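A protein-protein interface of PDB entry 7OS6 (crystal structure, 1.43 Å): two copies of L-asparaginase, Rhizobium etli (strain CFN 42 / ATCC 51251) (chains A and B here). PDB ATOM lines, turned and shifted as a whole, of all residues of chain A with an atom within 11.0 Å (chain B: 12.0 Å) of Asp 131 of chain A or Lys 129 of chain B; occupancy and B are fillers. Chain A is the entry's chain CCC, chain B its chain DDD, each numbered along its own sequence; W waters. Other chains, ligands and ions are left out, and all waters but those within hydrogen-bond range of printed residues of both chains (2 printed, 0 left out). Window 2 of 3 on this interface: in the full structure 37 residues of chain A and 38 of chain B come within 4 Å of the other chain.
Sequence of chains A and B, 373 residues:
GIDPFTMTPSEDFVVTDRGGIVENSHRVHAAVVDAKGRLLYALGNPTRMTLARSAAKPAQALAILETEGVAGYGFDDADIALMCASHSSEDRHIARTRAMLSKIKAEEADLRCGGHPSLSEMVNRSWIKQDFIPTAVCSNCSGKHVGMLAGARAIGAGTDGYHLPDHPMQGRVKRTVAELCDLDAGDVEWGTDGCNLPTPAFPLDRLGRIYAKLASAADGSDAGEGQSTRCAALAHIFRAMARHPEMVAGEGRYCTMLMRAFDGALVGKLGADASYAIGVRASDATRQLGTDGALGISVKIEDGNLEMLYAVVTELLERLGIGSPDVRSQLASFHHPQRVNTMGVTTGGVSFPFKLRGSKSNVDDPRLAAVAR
Asp 131 of chain A touches one residue of chain B. Printed residues of chain A within 4 Å of Lys 129 of chain B: Ile 128 (3.6 Å), Lys 129 (3.2 Å) and Asp 131 (2.9 Å). Of chain B, only Ile 128 (3.4 Å), Lys 129 (3.2 Å) and Asp 131 (2.9 Å) come within 4 Å of Lys 129 of chain A. No residue of chain B comes within 4 Å of Gln 130 of chain A. No residue of chain B comes within 4 Å of Phe 132 of chain A. No residue of chain B comes within 4 Å of Ile 133 of chain A. No residue of chain A comes within 4 Å of Ser 126 of chain B. Of chain A, only Arg 125 (3.6 Å), Ile 128 (3.7 Å) and Lys 129 (3.4 Å) come within 4 Å of Ile 128 of chain B. Gln 130 of chain B touches none of the printed residues of chain A. Of the printed residues of chain A, Arg 125 of chain B touches Ile 128. Printed residues of chain B within 4 Å of Arg 125 of chain A: Ile 128. Printed residues of chain A within 4 Å of Asp 131 of chain B: Lys 129 (2.9 Å). Asn 124 of chain A touches none of the printed residues of chain B. The nearest residue of chain B that does not touch Asp 131 of chain A is Arg 125 of chain B (6.4 Å). The nearest printed residue of chain B that does not touch Arg 125 of chain A is Asn 124 of chain B (4.7 Å).
The guanidinium group (NH2) of Arg 125 of chain B lies within salt-bridge range of the side-chain carboxylate (OE2) of Glu 121 of chain B (3.3 Å).
Water W2 lies within hydrogen-bond range of OD1 of Asn 124 of chain B (2.8 Å) and NH2 of Arg 125 of chain A (3.3 Å). Water W1 bridges the side-chain amide nitrogen of Asn 124 of chain A (2.9 Å) and the guanidinium group of Arg 125 of chain B (3.0 Å).
Printed residues of chain B that touch a printed residue of chain A: Arg 125, Ile 128, Lys 129 and Asp 131. Of the 14 printed residues of chain A, 4 touch a printed residue of chain B. Printed residues of chain A that touch a printed residue of chain B: Arg 125, Ile 128, Lys 129 and Asp 131. Hydrophobic or aromatic side chains of chain A that line the printed part of chain B: Ile 128. Among the printed residues, Asp or Glu carboxylates within 4 Å of a Lys or Arg side-chain nitrogen of the other chain: Lys 129 of chain A with Asp 131 of chain B (2.9 Å) and Asp 131 of chain A with Lys 129 of chain B (2.9 Å).
Among the printed residues, pairs that only touch across the chains: Arg 125 of chain A with Ile 128 of chain B, Ile 128 of chain A with Arg 125 of chain B, Ile 128 of chain A with Ile 128 of chain B, Ile 128 of chain A with Lys 129 of chain B, Lys 129 of chain A with Ile 128 of chain B and Lys 129 of chain A with Lys 129 of chain B.
Ile 128 of chain A touches its own counterpart, Ile 128 of chain B. Ile 128 of chain A touches Lys 129 of chain B, and with the chains exchanged Lys 129 of chain A touches Ile 128 of chain B. Lys 129 of chain A touches its own counterpart, Lys 129 of chain B. Lys 129 of chain A touches Asp 131 of chain B, and with the chains exchanged Asp 131 of chain A touches Lys 129 of chain B. Of the 8 pairs that touch across the chains among the printed residues, 8 have their exchanged pair printed and touching as well.
The side-chain carboxylate (OD2) of Asp 131 of chain B is in salt-bridge range of the side-chain amino group (NZ) of Lys 129 of chain A, at 2.9 Å. The side-chain carboxylate (OD2) of Asp 131 of chain A lies within salt-bridge range of the side-chain amino group (NZ) of Lys 129 of chain B.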
ATOM      1  N   VAL A 123      21.044  22.793   8.447  1.00  0.00           N
ATOM      2  CA  VAL A 123      22.496  22.882   8.144  1.00  0.00           C
ATOM      3  C   VAL A 123      22.990  21.556   7.567  1.00  0.00           C
ATOM      4  O   VAL A 123      23.732  21.555   6.593  1.00  0.00           O
ATOM      5  CB  VAL A 123      23.320  23.257   9.400  1.00  0.00           C
ATOM      6  CG1 VAL A 123      24.812  23.164   9.127  1.00  0.00           C
ATOM      7  CG2 VAL A 123      22.910  24.611   9.930  1.00  0.00           C
ATOM      8  N   ASN A 124      22.613  20.448   8.193  1.00  0.00           N
ATOM      9  CA  ASN A 124      23.101  19.114   7.780  1.00  0.00           C
ATOM     10  C   ASN A 124      22.643  18.835   6.350  1.00  0.00           C
ATOM     11  O   ASN A 124      23.452  18.287   5.575  1.00  0.00           O
ATOM     12  CB  ASN A 124      22.691  18.063   8.814  1.00  0.00           C
ATOM     13  CG  ASN A 124      23.694  16.951   8.894  1.00  0.00           C
ATOM     14  OD1 ASN A 124      24.900  17.194   9.044  1.00  0.00           O
ATOM     15  ND2 ASN A 124      23.214  15.731   8.669  1.00  0.00           N
ATOM     16  N   ARG A 125      21.423  19.231   6.001  1.00  0.00           N
ATOM     17  CA  ARG A 125      20.895  19.095   4.613  1.00  0.00           C
ATOM     18  C   ARG A 125      21.817  19.819   3.637  1.00  0.00           C
ATOM     19  O   ARG A 125      22.190  19.215   2.637  1.00  0.00           O
ATOM     20  CB  ARG A 125      19.458  19.617   4.535  1.00  0.00           C
ATOM     21  CG  ARG A 125      18.440  18.600   5.027  1.00  0.00           C
ATOM     22  CD  ARG A 125      16.991  19.018   4.818  1.00  0.00           C
ATOM     23  NE  ARG A 125      16.102  17.872   4.651  1.00  0.00           N
ATOM     24  CZ  ARG A 125      15.550  17.472   3.498  1.00  0.00           C
ATOM     25  NH1 ARG A 125      15.794  18.138   2.377  1.00  0.00           N
ATOM     26  NH2 ARG A 125      14.763  16.409   3.473  1.00  0.00           N
ATOM     27  N   SER A 126      22.222  21.053   3.943  1.00  0.00           N
ATOM     28  CA  SER A 126      23.143  21.858   3.102  1.00  0.00           C
ATOM     29  C   SER A 126      24.494  21.148   2.978  1.00  0.00           C
ATOM     30  O   SER A 126      25.071  21.110   1.877  1.00  0.00           O
ATOM     31  CB  SER A 126      23.298  23.263   3.623  1.00  0.00           C
ATOM     32  OG  SER A 126      23.989  23.304   4.869  1.00  0.00           O
ATOM     33  N   TRP A 127      25.003  20.594   4.081  1.00  0.00           N
ATOM     34  CA  TRP A 127      26.277  19.844   4.059  1.00  0.00           C
ATOM     35  C   TRP A 127      26.159  18.613   3.148  1.00  0.00           C
ATOM     36  O   TRP A 127      27.101  18.343   2.415  1.00  0.00           O
ATOM     37  CB  TRP A 127      26.643  19.415   5.486  1.00  0.00           C
ATOM     38  CG  TRP A 127      27.091  20.548   6.355  1.00  0.00           C
ATOM     39  CD1 TRP A 127      27.144  21.884   6.067  1.00  0.00           C
ATOM     40  CD2 TRP A 127      27.561  20.406   7.701  1.00  0.00           C
ATOM     41  NE1 TRP A 127      27.636  22.584   7.156  1.00  0.00           N
ATOM     42  CE2 TRP A 127      27.902  21.694   8.157  1.00  0.00           C
ATOM     43  CE3 TRP A 127      27.801  19.299   8.520  1.00  0.00           C
ATOM     44  CZ2 TRP A 127      28.430  21.899   9.433  1.00  0.00           C
ATOM     45  CZ3 TRP A 127      28.294  19.501   9.788  1.00  0.00           C
ATOM     46  CH2 TRP A 127      28.588  20.794  10.239  1.00  0.00           C
ATOM     47  N   ILE A 128      25.070  17.865   3.276  1.00  0.00           N
ATOM     48  CA  ILE A 128      24.879  16.607   2.494  1.00  0.00           C
ATOM     49  C   ILE A 128      24.863  16.985   1.010  1.00  0.00           C
ATOM     50  O   ILE A 128      25.584  16.329   0.220  1.00  0.00           O
ATOM     51  CB  ILE A 128      23.607  15.868   2.936  1.00  0.00           C
ATOM     52  CG1 ILE A 128      23.782  15.244   4.319  1.00  0.00           C
ATOM     53  CG2 ILE A 128      23.238  14.824   1.894  1.00  0.00           C
ATOM     54  CD1 ILE A 128      22.500  14.888   5.029  1.00  0.00           C
ATOM     55  N   LYS A 129      24.123  18.037   0.655  1.00  0.00           N
ATOM     56  CA  LYS A 129      23.992  18.521  -0.744  1.00  0.00           C
ATOM     57  C   LYS A 129      25.371  18.898  -1.298  1.00  0.00           C
ATOM     58  O   LYS A 129      25.590  18.662  -2.492  1.00  0.00           O
ATOM     59  CB  LYS A 129      22.993  19.682  -0.796  1.00  0.00           C
ATOM     60  CG  LYS A 129      22.602  20.177  -2.171  1.00  0.00           C
ATOM     61  CD  LYS A 129      21.232  19.749  -2.595  1.00  0.00           C
ATOM     62  CE  LYS A 129      21.081  19.759  -4.098  1.00  0.00           C
ATOM     63  NZ  LYS A 129      20.884  21.134  -4.606  1.00  0.00           N
ATOM     64  N   GLN A 130      26.286  19.428  -0.472  1.00  0.00           N
ATOM     65  CA  GLN A 130      27.612  19.930  -0.926  1.00  0.00           C
ATOM     66  C   GLN A 130      28.721  18.892  -0.699  1.00  0.00           C
ATOM     67  O   GLN A 130      29.867  19.230  -0.969  1.00  0.00           O
ATOM     68  CB  GLN A 130      27.946  21.253  -0.238  1.00  0.00           C
ATOM     69  CG  GLN A 130      26.924  22.354  -0.505  1.00  0.00           C
ATOM     70  CD  GLN A 130      27.144  23.561   0.379  1.00  0.00           C
ATOM     71  OE1 GLN A 130      28.282  23.967   0.613  1.00  0.00           O
ATOM     72  NE2 GLN A 130      26.065  24.155   0.881  1.00  0.00           N
ATOM     73  N   ASP A 131      28.395  17.692  -0.209  1.00  0.00           N
ATOM     74  CA  ASP A 131      29.369  16.637   0.195  1.00  0.00           C
ATOM     75  C   ASP A 131      30.399  17.211   1.183  1.00  0.00           C
ATOM     76  O   ASP A 131      31.588  16.854   1.083  1.00  0.00           O
ATOM     77  CB  ASP A 131      30.092  16.046  -1.013  1.00  0.00           C
ATOM     78  CG  ASP A 131      29.158  15.281  -1.934  1.00  0.00           C
ATOM     79  OD1 ASP A 131      28.424  14.403  -1.433  1.00  0.00           O
ATOM     80  OD2 ASP A 131      29.174  15.584  -3.133  1.00  0.00           O
ATOM     81  N   PHE A 132      29.960  18.071   2.100  1.00  0.00           N
ATOM     82  CA  PHE A 132      30.870  18.704   3.099  1.00  0.00           C
ATOM     83  C   PHE A 132      31.206  17.690   4.197  1.00  0.00           C
ATOM     84  O   PHE A 132      30.277  17.082   4.751  1.00  0.00           O
ATOM     85  CB  PHE A 132      30.238  19.979   3.659  1.00  0.00           C
ATOM     86  CG  PHE A 132      31.092  20.644   4.714  1.00  0.00           C
ATOM     87  CD1 PHE A 132      32.327  21.193   4.395  1.00  0.00           C
ATOM     88  CD2 PHE A 132      30.705  20.642   6.035  1.00  0.00           C
ATOM     89  CE1 PHE A 132      33.137  21.777   5.363  1.00  0.00           C
ATOM     90  CE2 PHE A 132      31.497  21.250   6.998  1.00  0.00           C
ATOM     91  CZ  PHE A 132      32.725  21.776   6.676  1.00  0.00           C
ATOM     92  N   ILE A 133      32.495  17.517   4.509  1.00  0.00           N
ATOM     93  CA  ILE A 133      32.977  16.668   5.630  1.00  0.00           C
ATOM     94  C   ILE A 133      33.352  17.618   6.765  1.00  0.00           C
ATOM     95  O   ILE A 133      34.305  18.377   6.645  1.00  0.00           O
ATOM     96  CB  ILE A 133      34.155  15.772   5.205  1.00  0.00           C
ATOM     97  CG1 ILE A 133      33.767  14.869   4.022  1.00  0.00           C
ATOM     98  CG2 ILE A 133      34.666  14.955   6.379  1.00  0.00           C
ATOM     99  CD1 ILE A 133      32.647  13.899   4.338  1.00  0.00           C
ATOM    100  N   PRO A 134      32.605  17.637   7.889  1.00  0.00           N
ATOM    101  CA  PRO A 134      32.947  18.537   8.985  1.00  0.00           C
ATOM    102  C   PRO A 134      34.280  18.154   9.627  1.00  0.00           C
ATOM    103  O   PRO A 134      34.631  16.985   9.720  1.00  0.00           O
ATOM    104  CB  PRO A 134      31.757  18.417   9.951  1.00  0.00           C
ATOM    105  CG  PRO A 134      31.152  17.113   9.631  1.00  0.00           C
ATOM    106  CD  PRO A 134      31.422  16.818   8.182  1.00  0.00           C
ATOM    107  N   THR A 135      34.977  19.181  10.101  1.00  0.00           N
ATOM    108  CA  THR A 135      36.296  19.043  10.746  1.00  0.00           C
ATOM    109  C   THR A 135      36.213  19.576  12.184  1.00  0.00           C
ATOM    110  O   THR A 135      35.121  19.982  12.634  1.00  0.00           O
ATOM    111  CB  THR A 135      37.377  19.719   9.896  1.00  0.00           C
ATOM    112  OG1 THR A 135      37.077  21.104   9.890  1.00  0.00           O
ATOM    113  CG2 THR A 135      37.462  19.181   8.479  1.00  0.00           C
ATOM    114  N   CYS A 138      34.254  22.685  13.263  1.00  0.00           N
ATOM    115  CA  CYS A 138      32.788  22.512  13.118  1.00  0.00           C
ATOM    116  C   CYS A 138      32.149  21.883  14.356  1.00  0.00           C
ATOM    117  O   CYS A 138      30.915  21.890  14.409  1.00  0.00           O
ATOM    118  CB  CYS A 138      32.455  21.673  11.908  1.00  0.00           C
ATOM    119  SG  CYS A 138      33.066  22.355  10.351  1.00  0.00           S
ATOM    120  N   PRO B 117      10.411  11.338   4.565  1.00  0.00           N
ATOM    121  CA  PRO B 117      11.823  11.010   4.448  1.00  0.00           C
ATOM    122  C   PRO B 117      12.040   9.494   4.572  1.00  0.00           C
ATOM    123  O   PRO B 117      11.380   8.833   5.379  1.00  0.00           O
ATOM    124  CB  PRO B 117      12.460  11.779   5.612  1.00  0.00           C
ATOM    125  CG  PRO B 117      11.493  12.894   5.882  1.00  0.00           C
ATOM    126  CD  PRO B 117      10.115  12.315   5.627  1.00  0.00           C
ATOM    127  N   SER B 118      12.995   8.975   3.807  1.00  0.00           N
ATOM    128  CA  SER B 118      13.247   7.525   3.740  1.00  0.00           C
ATOM    129  C   SER B 118      13.608   6.985   5.131  1.00  0.00           C
ATOM    130  O   SER B 118      14.339   7.676   5.896  1.00  0.00           O
ATOM    131  CB  SER B 118      14.326   7.197   2.739  1.00  0.00           C
ATOM    132  OG  SER B 118      14.714   5.843   2.874  1.00  0.00           O
ATOM    133  N   SER B 120      15.733   4.754   5.392  1.00  0.00           N
ATOM    134  CA  SER B 120      17.182   4.497   5.197  1.00  0.00           C
ATOM    135  C   SER B 120      17.935   5.821   5.147  1.00  0.00           C
ATOM    136  O   SER B 120      17.660   6.634   4.262  1.00  0.00           O
ATOM    137  CB  SER B 120      17.409   3.720   3.936  1.00  0.00           C
ATOM    138  OG  SER B 120      18.793   3.698   3.597  1.00  0.00           O
ATOM    139  N   GLU B 121      18.948   5.993   6.013  1.00  0.00           N
ATOM    140  CA  GLU B 121      19.790   7.218   5.945  1.00  0.00           C
ATOM    141  C   GLU B 121      20.447   7.343   4.563  1.00  0.00           C
ATOM    142  O   GLU B 121      20.520   8.458   4.038  1.00  0.00           O
ATOM    143  CB  GLU B 121      20.865   7.193   7.045  1.00  0.00           C
ATOM    144  CG  GLU B 121      21.829   8.353   6.934  1.00  0.00           C
ATOM    145  CD  GLU B 121      22.920   8.401   7.996  1.00  0.00           C
ATOM    146  OE1 GLU B 121      23.184   7.354   8.628  1.00  0.00           O
ATOM    147  OE2 GLU B 121      23.529   9.537   8.185  1.00  0.00           O
ATOM    148  N   MET B 122      20.920   6.244   3.970  1.00  0.00           N
ATOM    149  CA  MET B 122      21.660   6.322   2.688  1.00  0.00           C
ATOM    150  C   MET B 122      20.708   6.704   1.555  1.00  0.00           C
ATOM    151  O   MET B 122      21.084   7.470   0.692  1.00  0.00           O
ATOM    152  CB  MET B 122      22.401   5.015   2.393  1.00  0.00           C
ATOM    153  CG  MET B 122      23.674   4.860   3.238  1.00  0.00           C
ATOM    154  SD  MET B 122      24.735   6.361   3.413  1.00  0.00           S
ATOM    155  CE  MET B 122      25.156   6.649   1.696  1.00  0.00           C
ATOM    156  N   VAL B 123      19.470   6.210   1.562  1.00  0.00           N
ATOM    157  CA  VAL B 123      18.473   6.621   0.540  1.00  0.00           C
ATOM    158  C   VAL B 123      18.172   8.100   0.725  1.00  0.00           C
ATOM    159  O   VAL B 123      18.119   8.826  -0.255  1.00  0.00           O
ATOM    160  CB  VAL B 123      17.182   5.785   0.625  1.00  0.00           C
ATOM    161  CG1 VAL B 123      16.099   6.335  -0.289  1.00  0.00           C
ATOM    162  CG2 VAL B 123      17.471   4.323   0.332  1.00  0.00           C
ATOM    163  N   ASN B 124      17.926   8.528   1.954  1.00  0.00           N
ATOM    164  CA  ASN B 124      17.522   9.921   2.228  1.00  0.00           C
ATOM    165  C   ASN B 124      18.657  10.860   1.789  1.00  0.00           C
ATOM    166  O   ASN B 124      18.358  11.913   1.225  1.00  0.00           O
ATOM    167  CB  ASN B 124      17.102  10.055   3.696  1.00  0.00           C
ATOM    168  CG  ASN B 124      16.043  11.110   3.870  1.00  0.00           C
ATOM    169  OD1 ASN B 124      15.015  11.096   3.190  1.00  0.00           O
ATOM    170  ND2 ASN B 124      16.335  12.110   4.693  1.00  0.00           N
ATOM    171  N   ARG B 125      19.914  10.469   1.993  1.00  0.00           N
ATOM    172  CA  ARG B 125      21.099  11.237   1.540  1.00  0.00           C
ATOM    173  C   ARG B 125      21.041  11.425   0.026  1.00  0.00           C
ATOM    174  O   ARG B 125      21.202  12.549  -0.422  1.00  0.00           O
ATOM    175  CB  ARG B 125      22.391  10.532   1.970  1.00  0.00           C
ATOM    176  CG  ARG B 125      23.677  11.239   1.569  1.00  0.00           C
ATOM    177  CD  ARG B 125      24.891  10.640   2.281  1.00  0.00           C
ATOM    178  NE  ARG B 125      24.745  10.609   3.744  1.00  0.00           N
ATOM    179  CZ  ARG B 125      25.324  11.445   4.611  1.00  0.00           C
ATOM    180  NH1 ARG B 125      26.130  12.401   4.175  1.00  0.00           N
ATOM    181  NH2 ARG B 125      25.093  11.320   5.906  1.00  0.00           N
ATOM    182  N   SER B 126      20.760  10.364  -0.740  1.00  0.00           N
ATOM    183  CA  SER B 126      20.622  10.431  -2.216  1.00  0.00           C
ATOM    184  C   SER B 126      19.471  11.371  -2.594  1.00  0.00           C
ATOM    185  O   SER B 126      19.610  12.158  -3.535  1.00  0.00           O
ATOM    186  CB  SER B 126      20.433   9.059  -2.804  1.00  0.00           C
ATOM    187  OG  SER B 126      20.343   9.115  -4.214  1.00  0.00           O
ATOM    188  N   TRP B 127      18.347  11.307  -1.878  1.00  0.00           N
ATOM    189  CA  TRP B 127      17.195  12.193  -2.138  1.00  0.00           C
ATOM    190  C   TRP B 127      17.597  13.658  -1.906  1.00  0.00           C
ATOM    191  O   TRP B 127      17.220  14.506  -2.708  1.00  0.00           O
ATOM    192  CB  TRP B 127      16.021  11.797  -1.251  1.00  0.00           C
ATOM    193  CG  TRP B 127      15.365  10.512  -1.661  1.00  0.00           C
ATOM    194  CD1 TRP B 127      15.721   9.630  -2.636  1.00  0.00           C
ATOM    195  CD2 TRP B 127      14.207   9.953  -1.022  1.00  0.00           C
ATOM    196  NE1 TRP B 127      14.832   8.575  -2.674  1.00  0.00           N
ATOM    197  CE2 TRP B 127      13.896   8.754  -1.695  1.00  0.00           C
ATOM    198  CE3 TRP B 127      13.401  10.373   0.033  1.00  0.00           C
ATOM    199  CZ2 TRP B 127      12.800   7.979  -1.327  1.00  0.00           C
ATOM    200  CZ3 TRP B 127      12.335   9.596   0.413  1.00  0.00           C
ATOM    201  CH2 TRP B 127      12.043   8.414  -0.264  1.00  0.00           C
ATOM    202  N   ILE B 128      18.278  13.925  -0.797  1.00  0.00           N
ATOM    203  CA  ILE B 128      18.675  15.317  -0.422  1.00  0.00           C
ATOM    204  C   ILE B 128      19.588  15.860  -1.523  1.00  0.00           C
ATOM    205  O   ILE B 128      19.331  16.988  -1.997  1.00  0.00           O
ATOM    206  CB  ILE B 128      19.327  15.345   0.970  1.00  0.00           C
ATOM    207  CG1 ILE B 128      18.278  15.110   2.059  1.00  0.00           C
ATOM    208  CG2 ILE B 128      20.075  16.664   1.163  1.00  0.00           C
ATOM    209  CD1 ILE B 128      18.828  14.691   3.409  1.00  0.00           C
ATOM    210  N   LYS B 129      20.566  15.060  -1.952  1.00  0.00           N
ATOM    211  CA  LYS B 129      21.545  15.437  -3.005  1.00  0.00           C
ATOM    212  C   LYS B 129      20.808  15.769  -4.307  1.00  0.00           C
ATOM    213  O   LYS B 129      21.268  16.679  -5.008  1.00  0.00           O
ATOM    214  CB  LYS B 129      22.594  14.336  -3.207  1.00  0.00           C
ATOM    215  CG  LYS B 129      23.706  14.326  -2.170  1.00  0.00           C
ATOM    216  CD  LYS B 129      24.873  13.415  -2.500  1.00  0.00           C
ATOM    217  CE  LYS B 129      25.711  13.870  -3.678  1.00  0.00           C
ATOM    218  NZ  LYS B 129      26.279  15.229  -3.489  1.00  0.00           N
ATOM    219  N   GLN B 130      19.700  15.084  -4.623  1.00  0.00           N
ATOM    220  CA  GLN B 130      18.980  15.242  -5.920  1.00  0.00           C
ATOM    221  C   GLN B 130      17.773  16.182  -5.779  1.00  0.00           C
ATOM    222  O   GLN B 130      17.054  16.329  -6.777  1.00  0.00           O
ATOM    223  CB  GLN B 130      18.546  13.881  -6.464  1.00  0.00           C
ATOM    224  CG  GLN B 130      19.705  12.922  -6.705  1.00  0.00           C
ATOM    225  CD  GLN B 130      19.244  11.509  -6.979  1.00  0.00           C
ATOM    226  OE1 GLN B 130      18.223  11.286  -7.624  1.00  0.00           O
ATOM    227  NE2 GLN B 130      19.990  10.537  -6.478  1.00  0.00           N
ATOM    228  N   ASP B 131      17.555  16.788  -4.612  1.00  0.00           N
ATOM    229  CA  ASP B 131      16.365  17.623  -4.288  1.00  0.00           C
ATOM    230  C   ASP B 131      15.066  16.852  -4.581  1.00  0.00           C
ATOM    231  O   ASP B 131      14.105  17.456  -5.091  1.00  0.00           O
ATOM    232  CB  ASP B 131      16.385  18.938  -5.062  1.00  0.00           C
ATOM    233  CG  ASP B 131      17.523  19.838  -4.624  1.00  0.00           C
ATOM    234  OD1 ASP B 131      17.641  20.083  -3.410  1.00  0.00           O
ATOM    235  OD2 ASP B 131      18.280  20.278  -5.496  1.00  0.00           O
ATOM    236  N   PHE B 132      15.040  15.558  -4.289  1.00  0.00           N
ATOM    237  CA  PHE B 132      13.842  14.714  -4.550  1.00  0.00           C
ATOM    238  C   PHE B 132      12.793  14.962  -3.456  1.00  0.00           C
ATOM    239  O   PHE B 132      13.153  14.885  -2.269  1.00  0.00           O
ATOM    240  CB  PHE B 132      14.250  13.240  -4.648  1.00  0.00           C
ATOM    241  CG  PHE B 132      13.068  12.329  -4.879  1.00  0.00           C
ATOM    242  CD1 PHE B 132      12.319  12.406  -6.044  1.00  0.00           C
ATOM    243  CD2 PHE B 132      12.665  11.463  -3.877  1.00  0.00           C
ATOM    244  CE1 PHE B 132      11.210  11.596  -6.234  1.00  0.00           C
ATOM    245  CE2 PHE B 132      11.586  10.618  -4.093  1.00  0.00           C
ATOM    246  CZ  PHE B 132      10.846  10.702  -5.251  1.00  0.00           C
ATOM    247  N   ILE B 133      11.541  15.227  -3.831  1.00  0.00           N
ATOM    248  CA  ILE B 133      10.395  15.332  -2.880  1.00  0.00           C
ATOM    249  C   ILE B 133       9.621  14.016  -2.957  1.00  0.00           C
ATOM    250  O   ILE B 133       9.016  13.720  -3.976  1.00  0.00           O
ATOM    251  CB  ILE B 133       9.493  16.540  -3.208  1.00  0.00           C
ATOM    252  CG1 ILE B 133      10.280  17.858  -3.256  1.00  0.00           C
ATOM    253  CG2 ILE B 133       8.332  16.627  -2.234  1.00  0.00           C
ATOM    254  CD1 ILE B 133      10.937  18.229  -1.938  1.00  0.00           C
ATOM    255  N   PRO B 134       9.622  13.174  -1.906  1.00  0.00           N
ATOM    256  CA  PRO B 134       8.894  11.908  -1.975  1.00  0.00           C
ATOM    257  C   PRO B 134       7.389  12.138  -2.040  1.00  0.00           C
ATOM    258  O   PRO B 134       6.854  13.080  -1.461  1.00  0.00           O
ATOM    259  CB  PRO B 134       9.281  11.167  -0.694  1.00  0.00           C
ATOM    260  CG  PRO B 134       9.750  12.255   0.248  1.00  0.00           C
ATOM    261  CD  PRO B 134      10.309  13.367  -0.614  1.00  0.00           C
HETATM  262  O   HOH W   1      24.934  13.583   7.816  1.00  0.00           O
HETATM  263  O   HOH W   2      13.922  13.483   2.210  1.00  0.00           O
